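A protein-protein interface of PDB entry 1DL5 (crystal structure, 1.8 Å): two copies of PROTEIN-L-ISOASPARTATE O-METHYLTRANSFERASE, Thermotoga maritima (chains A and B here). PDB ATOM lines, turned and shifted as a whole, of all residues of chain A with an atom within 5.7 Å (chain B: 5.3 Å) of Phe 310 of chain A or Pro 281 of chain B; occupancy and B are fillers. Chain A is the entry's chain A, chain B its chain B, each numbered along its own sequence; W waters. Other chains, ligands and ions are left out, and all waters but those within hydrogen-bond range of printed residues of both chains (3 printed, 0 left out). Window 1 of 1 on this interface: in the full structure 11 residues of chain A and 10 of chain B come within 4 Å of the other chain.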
ATOM      1  N   TYR A 194       7.213   2.246 -26.397  1.00  0.00           N
ATOM      2  CA  TYR A 194       6.825   1.530 -27.606  1.00  0.00           C
ATOM      3  C   TYR A 194       7.384   2.059 -28.911  1.00  0.00           C
ATOM      4  O   TYR A 194       7.794   3.209 -29.019  1.00  0.00           O
ATOM      5  CB  TYR A 194       5.302   1.540 -27.797  1.00  0.00           C
ATOM      6  CG  TYR A 194       4.502   0.949 -26.666  1.00  0.00           C
ATOM      7  CD1 TYR A 194       4.105   1.737 -25.582  1.00  0.00           C
ATOM      8  CD2 TYR A 194       4.165  -0.403 -26.662  1.00  0.00           C
ATOM      9  CE1 TYR A 194       3.388   1.184 -24.514  1.00  0.00           C
ATOM     10  CE2 TYR A 194       3.453  -0.967 -25.596  1.00  0.00           C
ATOM     11  CZ  TYR A 194       3.071  -0.169 -24.530  1.00  0.00           C
ATOM     12  OH  TYR A 194       2.381  -0.727 -23.477  1.00  0.00           O
ATOM     13  N   ARG A 250       9.306 -12.994 -28.855  1.00  0.00           N
ATOM     14  CA  ARG A 250       9.587 -14.091 -27.933  1.00  0.00           C
ATOM     15  C   ARG A 250       9.138 -15.430 -28.503  1.00  0.00           C
ATOM     16  O   ARG A 250       9.004 -16.408 -27.768  1.00  0.00           O
ATOM     17  CB  ARG A 250       8.874 -13.858 -26.593  1.00  0.00           C
ATOM     18  CG  ARG A 250       9.519 -12.786 -25.729  1.00  0.00           C
ATOM     19  CD  ARG A 250       8.596 -12.386 -24.584  1.00  0.00           C
ATOM     20  NE  ARG A 250       9.320 -11.694 -23.526  1.00  0.00           N
ATOM     21  CZ  ARG A 250      10.049 -12.307 -22.596  1.00  0.00           C
ATOM     22  NH1 ARG A 250      10.146 -13.631 -22.583  1.00  0.00           N
ATOM     23  NH2 ARG A 250      10.687 -11.595 -21.677  1.00  0.00           N
ATOM     24  N   TYR A 260       5.363 -19.391 -27.562  1.00  0.00           N
ATOM     25  CA  TYR A 260       5.637 -18.037 -27.106  1.00  0.00           C
ATOM     26  C   TYR A 260       6.346 -18.313 -25.773  1.00  0.00           C
ATOM     27  O   TYR A 260       5.765 -18.947 -24.889  1.00  0.00           O
ATOM     28  CB  TYR A 260       4.339 -17.279 -26.835  1.00  0.00           C
ATOM     29  CG  TYR A 260       4.525 -16.092 -25.908  1.00  0.00           C
ATOM     30  CD1 TYR A 260       5.200 -14.946 -26.329  1.00  0.00           C
ATOM     31  CD2 TYR A 260       4.040 -16.126 -24.602  1.00  0.00           C
ATOM     32  CE1 TYR A 260       5.385 -13.858 -25.466  1.00  0.00           C
ATOM     33  CE2 TYR A 260       4.221 -15.045 -23.731  1.00  0.00           C
ATOM     34  CZ  TYR A 260       4.892 -13.921 -24.169  1.00  0.00           C
ATOM     35  OH  TYR A 260       5.059 -12.854 -23.311  1.00  0.00           O
ATOM     36  N   PRO A 263       7.516 -14.622 -19.822  1.00  0.00           N
ATOM     37  CA  PRO A 263       8.216 -14.537 -18.541  1.00  0.00           C
ATOM     38  C   PRO A 263       7.523 -15.334 -17.434  1.00  0.00           C
ATOM     39  O   PRO A 263       8.173 -15.782 -16.493  1.00  0.00           O
ATOM     40  CB  PRO A 263       8.234 -13.030 -18.262  1.00  0.00           C
ATOM     41  CG  PRO A 263       6.961 -12.552 -18.908  1.00  0.00           C
ATOM     42  CD  PRO A 263       6.956 -13.314 -20.217  1.00  0.00           C
ATOM     43  N   ASN A 264       6.214 -15.534 -17.558  1.00  0.00           N
ATOM     44  CA  ASN A 264       5.462 -16.241 -16.534  1.00  0.00           C
ATOM     45  C   ASN A 264       4.670 -17.417 -17.067  1.00  0.00           C
ATOM     46  O   ASN A 264       3.839 -17.995 -16.365  1.00  0.00           O
ATOM     47  CB  ASN A 264       4.518 -15.262 -15.841  1.00  0.00           C
ATOM     48  CG  ASN A 264       5.241 -14.026 -15.349  1.00  0.00           C
ATOM     49  OD1 ASN A 264       6.094 -14.107 -14.467  1.00  0.00           O
ATOM     50  ND2 ASN A 264       4.919 -12.879 -15.933  1.00  0.00           N
ATOM     51  N   PRO A 281      -1.236 -13.732 -19.560  1.00  0.00           N
ATOM     52  CA  PRO A 281      -2.327 -12.781 -19.773  1.00  0.00           C
ATOM     53  C   PRO A 281      -2.045 -11.806 -20.914  1.00  0.00           C
ATOM     54  O   PRO A 281      -2.973 -11.320 -21.554  1.00  0.00           O
ATOM     55  CB  PRO A 281      -2.447 -12.087 -18.418  1.00  0.00           C
ATOM     56  CG  PRO A 281      -1.046 -12.132 -17.891  1.00  0.00           C
ATOM     57  CD  PRO A 281      -0.638 -13.553 -18.225  1.00  0.00           C
ATOM     58  N   GLU A 282      -0.768 -11.527 -21.167  1.00  0.00           N
ATOM     59  CA  GLU A 282      -0.400 -10.605 -22.240  1.00  0.00           C
ATOM     60  C   GLU A 282      -0.786 -11.185 -23.606  1.00  0.00           C
ATOM     61  O   GLU A 282      -1.112 -10.439 -24.529  1.00  0.00           O
ATOM     62  CB  GLU A 282       1.108 -10.287 -22.202  1.00  0.00           C
ATOM     63  CG  GLU A 282       2.040 -11.471 -22.474  1.00  0.00           C
ATOM     64  CD  GLU A 282       2.432 -12.235 -21.224  1.00  0.00           C
ATOM     65  OE1 GLU A 282       1.649 -12.232 -20.247  1.00  0.00           O
ATOM     66  OE2 GLU A 282       3.523 -12.853 -21.226  1.00  0.00           O
ATOM     67  N   ASN A 285      -4.497 -10.860 -24.007  1.00  0.00           N
ATOM     68  CA  ASN A 285      -4.836  -9.490 -24.377  1.00  0.00           C
ATOM     69  C   ASN A 285      -4.637  -9.254 -25.868  1.00  0.00           C
ATOM     70  O   ASN A 285      -5.460  -8.599 -26.502  1.00  0.00           O
ATOM     71  CB  ASN A 285      -4.012  -8.477 -23.575  1.00  0.00           C
ATOM     72  CG  ASN A 285      -4.452  -8.385 -22.122  1.00  0.00           C
ATOM     73  OD1 ASN A 285      -5.567  -8.783 -21.771  1.00  0.00           O
ATOM     74  ND2 ASN A 285      -3.584  -7.844 -21.273  1.00  0.00           N
ATOM     75  N   HIS A 304       2.059  -1.903 -31.811  1.00  0.00           N
ATOM     76  CA  HIS A 304       2.645  -1.178 -30.692  1.00  0.00           C
ATOM     77  C   HIS A 304       3.578  -2.190 -30.033  1.00  0.00           C
ATOM     78  O   HIS A 304       3.158  -2.994 -29.196  1.00  0.00           O
ATOM     79  CB  HIS A 304       1.556  -0.723 -29.711  1.00  0.00           C
ATOM     80  CG  HIS A 304       0.491   0.135 -30.336  1.00  0.00           C
ATOM     81  ND1 HIS A 304       0.322   1.466 -30.016  1.00  0.00           N
ATOM     82  CD2 HIS A 304      -0.476  -0.159 -31.238  1.00  0.00           C
ATOM     83  CE1 HIS A 304      -0.704   1.954 -30.691  1.00  0.00           C
ATOM     84  NE2 HIS A 304      -1.207   0.988 -31.441  1.00  0.00           N
ATOM     85  N   VAL A 305       4.844  -2.149 -30.437  1.00  0.00           N
ATOM     86  CA  VAL A 305       5.864  -3.074 -29.951  1.00  0.00           C
ATOM     87  C   VAL A 305       6.483  -2.542 -28.668  1.00  0.00           C
ATOM     88  O   VAL A 305       7.170  -1.523 -28.663  1.00  0.00           O
ATOM     89  CB  VAL A 305       6.954  -3.270 -31.028  1.00  0.00           C
ATOM     90  CG1 VAL A 305       7.914  -4.387 -30.622  1.00  0.00           C
ATOM     91  CG2 VAL A 305       6.290  -3.582 -32.362  1.00  0.00           C
ATOM     92  N   GLY A 306       6.234  -3.247 -27.572  1.00  0.00           N
ATOM     93  CA  GLY A 306       6.738  -2.795 -26.293  1.00  0.00           C
ATOM     94  C   GLY A 306       8.135  -3.216 -25.905  1.00  0.00           C
ATOM     95  O   GLY A 306       8.574  -4.334 -26.181  1.00  0.00           O
ATOM     96  N   ASN A 308      10.250  -3.395 -22.518  1.00  0.00           N
ATOM     97  CA  ASN A 308      10.116  -3.366 -21.063  1.00  0.00           C
ATOM     98  C   ASN A 308       8.637  -3.127 -20.746  1.00  0.00           C
ATOM     99  O   ASN A 308       8.271  -2.636 -19.676  1.00  0.00           O
ATOM    100  CB  ASN A 308      10.998  -2.289 -20.433  1.00  0.00           C
ATOM    101  CG  ASN A 308      12.469  -2.626 -20.540  1.00  0.00           C
ATOM    102  OD1 ASN A 308      12.877  -3.747 -20.233  1.00  0.00           O
ATOM    103  ND2 ASN A 308      13.269  -1.667 -20.983  1.00  0.00           N
ATOM    104  N   ALA A 309       7.801  -3.485 -21.715  1.00  0.00           N
ATOM    105  CA  ALA A 309       6.346  -3.401 -21.618  1.00  0.00           C
ATOM    106  C   ALA A 309       5.820  -4.421 -22.625  1.00  0.00           C
ATOM    107  O   ALA A 309       6.505  -4.742 -23.599  1.00  0.00           O
ATOM    108  CB  ALA A 309       5.854  -2.009 -21.994  1.00  0.00           C
ATOM    109  N   PHE A 310       4.620  -4.942 -22.397  1.00  0.00           N
ATOM    110  CA  PHE A 310       4.060  -5.905 -23.337  1.00  0.00           C
ATOM    111  C   PHE A 310       3.513  -5.146 -24.542  1.00  0.00           C
ATOM    112  O   PHE A 310       3.293  -3.939 -24.475  1.00  0.00           O
ATOM    113  CB  PHE A 310       2.978  -6.748 -22.657  1.00  0.00           C
ATOM    114  CG  PHE A 310       3.528  -7.734 -21.657  1.00  0.00           C
ATOM    115  CD1 PHE A 310       4.513  -8.644 -22.033  1.00  0.00           C
ATOM    116  CD2 PHE A 310       3.070  -7.747 -20.338  1.00  0.00           C
ATOM    117  CE1 PHE A 310       5.039  -9.555 -21.115  1.00  0.00           C
ATOM    118  CE2 PHE A 310       3.589  -8.655 -19.410  1.00  0.00           C
ATOM    119  CZ  PHE A 310       4.574  -9.560 -19.799  1.00  0.00           C
ATOM    120  N   SER A 311       3.315  -5.849 -25.649  1.00  0.00           N
ATOM    121  CA  SER A 311       2.842  -5.214 -26.876  1.00  0.00           C
ATOM    122  C   SER A 311       1.333  -5.241 -27.052  1.00  0.00           C
ATOM    123  O   SER A 311       0.629  -6.001 -26.390  1.00  0.00           O
ATOM    124  CB  SER A 311       3.502  -5.894 -28.078  1.00  0.00           C
ATOM    125  OG  SER A 311       4.912  -5.828 -27.973  1.00  0.00           O
ATOM    126  N   HIS A 312       0.828  -4.388 -27.936  1.00  0.00           N
ATOM    127  CA  HIS A 312      -0.597  -4.379 -28.215  1.00  0.00           C
ATOM    128  C   HIS A 312      -0.916  -4.011 -29.656  1.00  0.00           C
ATOM    129  O   HIS A 312      -0.054  -3.525 -30.400  1.00  0.00           O
ATOM    130  CB  HIS A 312      -1.391  -3.496 -27.215  1.00  0.00           C
ATOM    131  CG  HIS A 312      -0.999  -2.049 -27.177  1.00  0.00           C
ATOM    132  ND1 HIS A 312       0.011  -1.569 -26.373  1.00  0.00           N
ATOM    133  CD2 HIS A 312      -1.549  -0.963 -27.775  1.00  0.00           C
ATOM    134  CE1 HIS A 312       0.066  -0.252 -26.471  1.00  0.00           C
ATOM    135  NE2 HIS A 312      -0.870   0.141 -27.316  1.00  0.00           N
ATOM    136  N   ASN B 229       4.440   3.485 -18.547  1.00  0.00           N
ATOM    137  CA  ASN B 229       3.681   2.908 -19.643  1.00  0.00           C
ATOM    138  C   ASN B 229       2.415   3.728 -19.863  1.00  0.00           C
ATOM    139  O   ASN B 229       2.305   4.482 -20.836  1.00  0.00           O
ATOM    140  CB  ASN B 229       3.319   1.458 -19.302  1.00  0.00           C
ATOM    141  CG  ASN B 229       2.613   0.740 -20.440  1.00  0.00           C
ATOM    142  OD1 ASN B 229       1.935   1.358 -21.261  1.00  0.00           O
ATOM    143  ND2 ASN B 229       2.751  -0.584 -20.476  1.00  0.00           N
ATOM    144  N   ASN B 264       6.860  -7.931 -13.694  1.00  0.00           N
ATOM    145  CA  ASN B 264       7.200  -7.227 -14.930  1.00  0.00           C
ATOM    146  C   ASN B 264       6.852  -5.745 -14.934  1.00  0.00           C
ATOM    147  O   ASN B 264       6.864  -5.099 -15.988  1.00  0.00           O
ATOM    148  CB  ASN B 264       6.496  -7.907 -16.098  1.00  0.00           C
ATOM    149  CG  ASN B 264       6.719  -9.403 -16.102  1.00  0.00           C
ATOM    150  OD1 ASN B 264       7.845  -9.870 -16.252  1.00  0.00           O
ATOM    151  ND2 ASN B 264       5.651 -10.158 -15.918  1.00  0.00           N
ATOM    152  N   ASP B 279       4.895  -3.267 -17.124  1.00  0.00           N
ATOM    153  CA  ASP B 279       3.581  -3.809 -17.427  1.00  0.00           C
ATOM    154  C   ASP B 279       3.048  -4.705 -16.306  1.00  0.00           C
ATOM    155  O   ASP B 279       3.813  -5.312 -15.557  1.00  0.00           O
ATOM    156  CB  ASP B 279       3.594  -4.583 -18.752  1.00  0.00           C
ATOM    157  CG  ASP B 279       2.331  -4.358 -19.565  1.00  0.00           C
ATOM    158  OD1 ASP B 279       1.238  -4.369 -18.969  1.00  0.00           O
ATOM    159  OD2 ASP B 279       2.417  -4.178 -20.799  1.00  0.00           O
ATOM    160  N   ALA B 280       1.730  -4.753 -16.190  1.00  0.00           N
ATOM    161  CA  ALA B 280       1.078  -5.563 -15.170  1.00  0.00           C
ATOM    162  C   ALA B 280      -0.292  -6.012 -15.665  1.00  0.00           C
ATOM    163  O   ALA B 280      -1.324  -5.597 -15.139  1.00  0.00           O
ATOM    164  CB  ALA B 280       0.940  -4.758 -13.875  1.00  0.00           C
ATOM    165  N   PRO B 281      -0.320  -6.869 -16.697  1.00  0.00           N
ATOM    166  CA  PRO B 281      -1.599  -7.347 -17.227  1.00  0.00           C
ATOM    167  C   PRO B 281      -2.411  -8.097 -16.170  1.00  0.00           C
ATOM    168  O   PRO B 281      -3.631  -8.178 -16.270  1.00  0.00           O
ATOM    169  CB  PRO B 281      -1.180  -8.243 -18.396  1.00  0.00           C
ATOM    170  CG  PRO B 281       0.195  -8.713 -17.998  1.00  0.00           C
ATOM    171  CD  PRO B 281       0.809  -7.452 -17.440  1.00  0.00           C
ATOM    172  N   GLU B 282      -1.725  -8.632 -15.164  1.00  0.00           N
ATOM    173  CA  GLU B 282      -2.400  -9.370 -14.096  1.00  0.00           C
ATOM    174  C   GLU B 282      -3.254  -8.417 -13.268  1.00  0.00           C
ATOM    175  O   GLU B 282      -4.308  -8.805 -12.761  1.00  0.00           O
ATOM    176  CB  GLU B 282      -1.385 -10.089 -13.190  1.00  0.00           C
ATOM    177  CG  GLU B 282      -0.455  -9.165 -12.417  1.00  0.00           C
ATOM    178  CD  GLU B 282       0.828  -8.847 -13.167  1.00  0.00           C
ATOM    179  OE1 GLU B 282       0.822  -8.847 -14.423  1.00  0.00           O
ATOM    180  OE2 GLU B 282       1.845  -8.588 -12.494  1.00  0.00           O
ATOM    181  N   ILE B 283      -2.798  -7.169 -13.135  1.00  0.00           N
ATOM    182  CA  ILE B 283      -3.543  -6.158 -12.392  1.00  0.00           C
ATOM    183  C   ILE B 283      -4.680  -5.650 -13.283  1.00  0.00           C
ATOM    184  O   ILE B 283      -5.796  -5.397 -12.821  1.00  0.00           O
ATOM    185  CB  ILE B 283      -2.634  -4.973 -11.999  1.00  0.00           C
ATOM    186  CG1 ILE B 283      -1.543  -5.453 -11.038  1.00  0.00           C
ATOM    187  CG2 ILE B 283      -3.473  -3.856 -11.364  1.00  0.00           C
ATOM    188  CD1 ILE B 283      -2.085  -6.073  -9.746  1.00  0.00           C
ATOM    189  N   GLU B 284      -4.371  -5.505 -14.568  1.00  0.00           N
ATOM    190  CA  GLU B 284      -5.336  -5.057 -15.563  1.00  0.00           C
ATOM    191  C   GLU B 284      -6.520  -6.033 -15.586  1.00  0.00           C
ATOM    192  O   GLU B 284      -7.676  -5.615 -15.707  1.00  0.00           O
ATOM    193  CB  GLU B 284      -4.638  -4.961 -16.936  1.00  0.00           C
ATOM    194  CG  GLU B 284      -3.581  -3.827 -17.001  1.00  0.00           C
ATOM    195  CD  GLU B 284      -2.497  -4.011 -18.080  1.00  0.00           C
ATOM    196  OE1 GLU B 284      -2.821  -4.107 -19.277  1.00  0.00           O
ATOM    197  OE2 GLU B 284      -1.300  -4.045 -17.725  1.00  0.00           O
ATOM    198  N   ASN B 285      -6.238  -7.328 -15.446  1.00  0.00           N
ATOM    199  CA  ASN B 285      -7.301  -8.338 -15.429  1.00  0.00           C
ATOM    200  C   ASN B 285      -8.104  -8.326 -14.138  1.00  0.00           C
ATOM    201  O   ASN B 285      -9.318  -8.539 -14.151  1.00  0.00           O
ATOM    202  CB  ASN B 285      -6.735  -9.746 -15.638  1.00  0.00           C
ATOM    203  CG  ASN B 285      -6.445 -10.041 -17.090  1.00  0.00           C
ATOM    204  OD1 ASN B 285      -7.031  -9.433 -17.981  1.00  0.00           O
ATOM    205  ND2 ASN B 285      -5.552 -10.992 -17.337  1.00  0.00           N
ATOM    206  N   LEU B 286      -7.430  -8.108 -13.012  1.00  0.00           N
ATOM    207  CA  LEU B 286      -8.143  -8.060 -11.746  1.00  0.00           C
ATOM    208  C   LEU B 286      -9.086  -6.868 -11.782  1.00  0.00           C
ATOM    209  O   LEU B 286     -10.212  -6.931 -11.286  1.00  0.00           O
ATOM    210  CB  LEU B 286      -7.169  -7.895 -10.571  1.00  0.00           C
ATOM    211  CG  LEU B 286      -6.395  -9.133 -10.122  1.00  0.00           C
ATOM    212  CD1 LEU B 286      -5.525  -8.778  -8.927  1.00  0.00           C
ATOM    213  CD2 LEU B 286      -7.377 -10.243  -9.752  1.00  0.00           C
HETATM  214  O   HOH W   1       8.253  -5.220 -18.159  1.00  0.00           O
HETATM  215  O   HOH W   2      -5.067  -7.792 -18.741  1.00  0.00           O
HETATM  216  O   HOH W   3       8.534 -12.294 -14.772  1.00  0.00           O
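The side-chain amide nitrogen (ND2) of Asn 229 of chain B lies within hydrogen-bond range of the side-chain hydroxyl (OH) of Tyr 194 of chain A, at 3.0 Å.
The side-chain amide nitrogen of Asn 264 of chain A lies close to the side-chain amide nitrogen of Asn 264 of chain B (2.8 Å).
N of Phe 310 of chain A sits at hydrogen-bond distance from OD2 of Asp 279 of chain B (2.8 Å).
O of Phe 310 of chain A sits close to OH of Tyr 194 of chain A (3.5 Å).
The backbone NH (N) of Asp 279 of chain B is in hydrogen-bond range of the backbone carbonyl oxygen (O) of Asn 264 of chain B.
Among the printed residues, merely in contact across the chains: Pro 281 of chain A with Asn 285 of chain B, Phe 310 of chain A with Pro 281 of chain B, Pro 281 of chain A with Pro 281 of chain B, Ala 309 of chain A with Asn 229 of chain B, Pro 263 of chain A with Asn 264 of chain B, Asn 285 of chain A with Pro 281 of chain B and Ala 309 of chain A with Asp 279 of chain B.
Of chain B, only Asp 279 (2.8 Å) and Pro 281 (3.6 Å) come within 4 Å of Phe 310 of chain A.
Of chain A, only Pro 281 (3.6 Å), Asn 285 (3.8 Å) and Phe 310 (3.6 Å) come within 4 Å of Pro 281 of chain B.
Of the printed residues of chain A, Asn 285 of chain B touches Pro 281.
Of the printed residues of chain B, Tyr 194 of chain A touches Asn 229 (3.0 Å).
Printed residues of chain A within 4 Å of Asn 264 of chain B: Pro 263 and Asn 264.
Of the printed residues of chain A, Asp 279 of chain B touches Ala 309 (3.9 Å) and Phe 310 (2.8 Å).
Of the printed residues of chain B, Pro 281 of chain A touches Pro 281 (3.6 Å) and Asn 285 (3.5 Å).
Glu 284 of chain B touches none of the printed residues of chain A.
The nearest residue of chain B that does not touch Phe 310 of chain A is Asn 264 of chain B (4.1 Å).
The nearest printed residue of chain B that does not touch Pro 263 of chain A is Pro 281 of chain B (7.8 Å).
Hydrophobic or aromatic side chains of chain B within 4 Å of the printed part of chain A: Pro 281.
Hydrophobic or aromatic side chains of chain A that line the printed part of chain B: Tyr 194, Pro 263, Pro 281, Ala 309 and Phe 310.
Among the printed residues, 10 pairs touch across the chains.
Among the printed residues, no Asp or Glu carboxylate lies within 4 Å of a Lys or Arg side-chain nitrogen of the other chain.
Asn 264 of chain B touches its own counterpart, Asn 264 of chain A.
Pro 281 of chain A touches its own counterpart, Pro 281 of chain B.
Pro 281 of chain A touches Asn 285 of chain B, and with the chains exchanged Asn 285 of chain A touches Pro 281 of chain B.
Of the 10 pairs that touch across the chains among the printed residues, 4 have their exchanged pair printed and touching as well.
Water W1 lies within hydrogen-bond range of the backbone carbonyl oxygen (O) of Asn 264 of chain B and the backbone carbonyl oxygen (O) of Asn 308 of chain A.
Water W2 lies within hydrogen-bond range of OD1 of Asn 285 of chain B, O of Pro 281 of chain B and ND2 of Asn 285 of chain A.
Water W3 lies within hydrogen-bond range of the side-chain amide oxygen (OD1) of Asn 264 of chain B and the side-chain amide oxygen (OD1) of Asn 264 of chain A.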
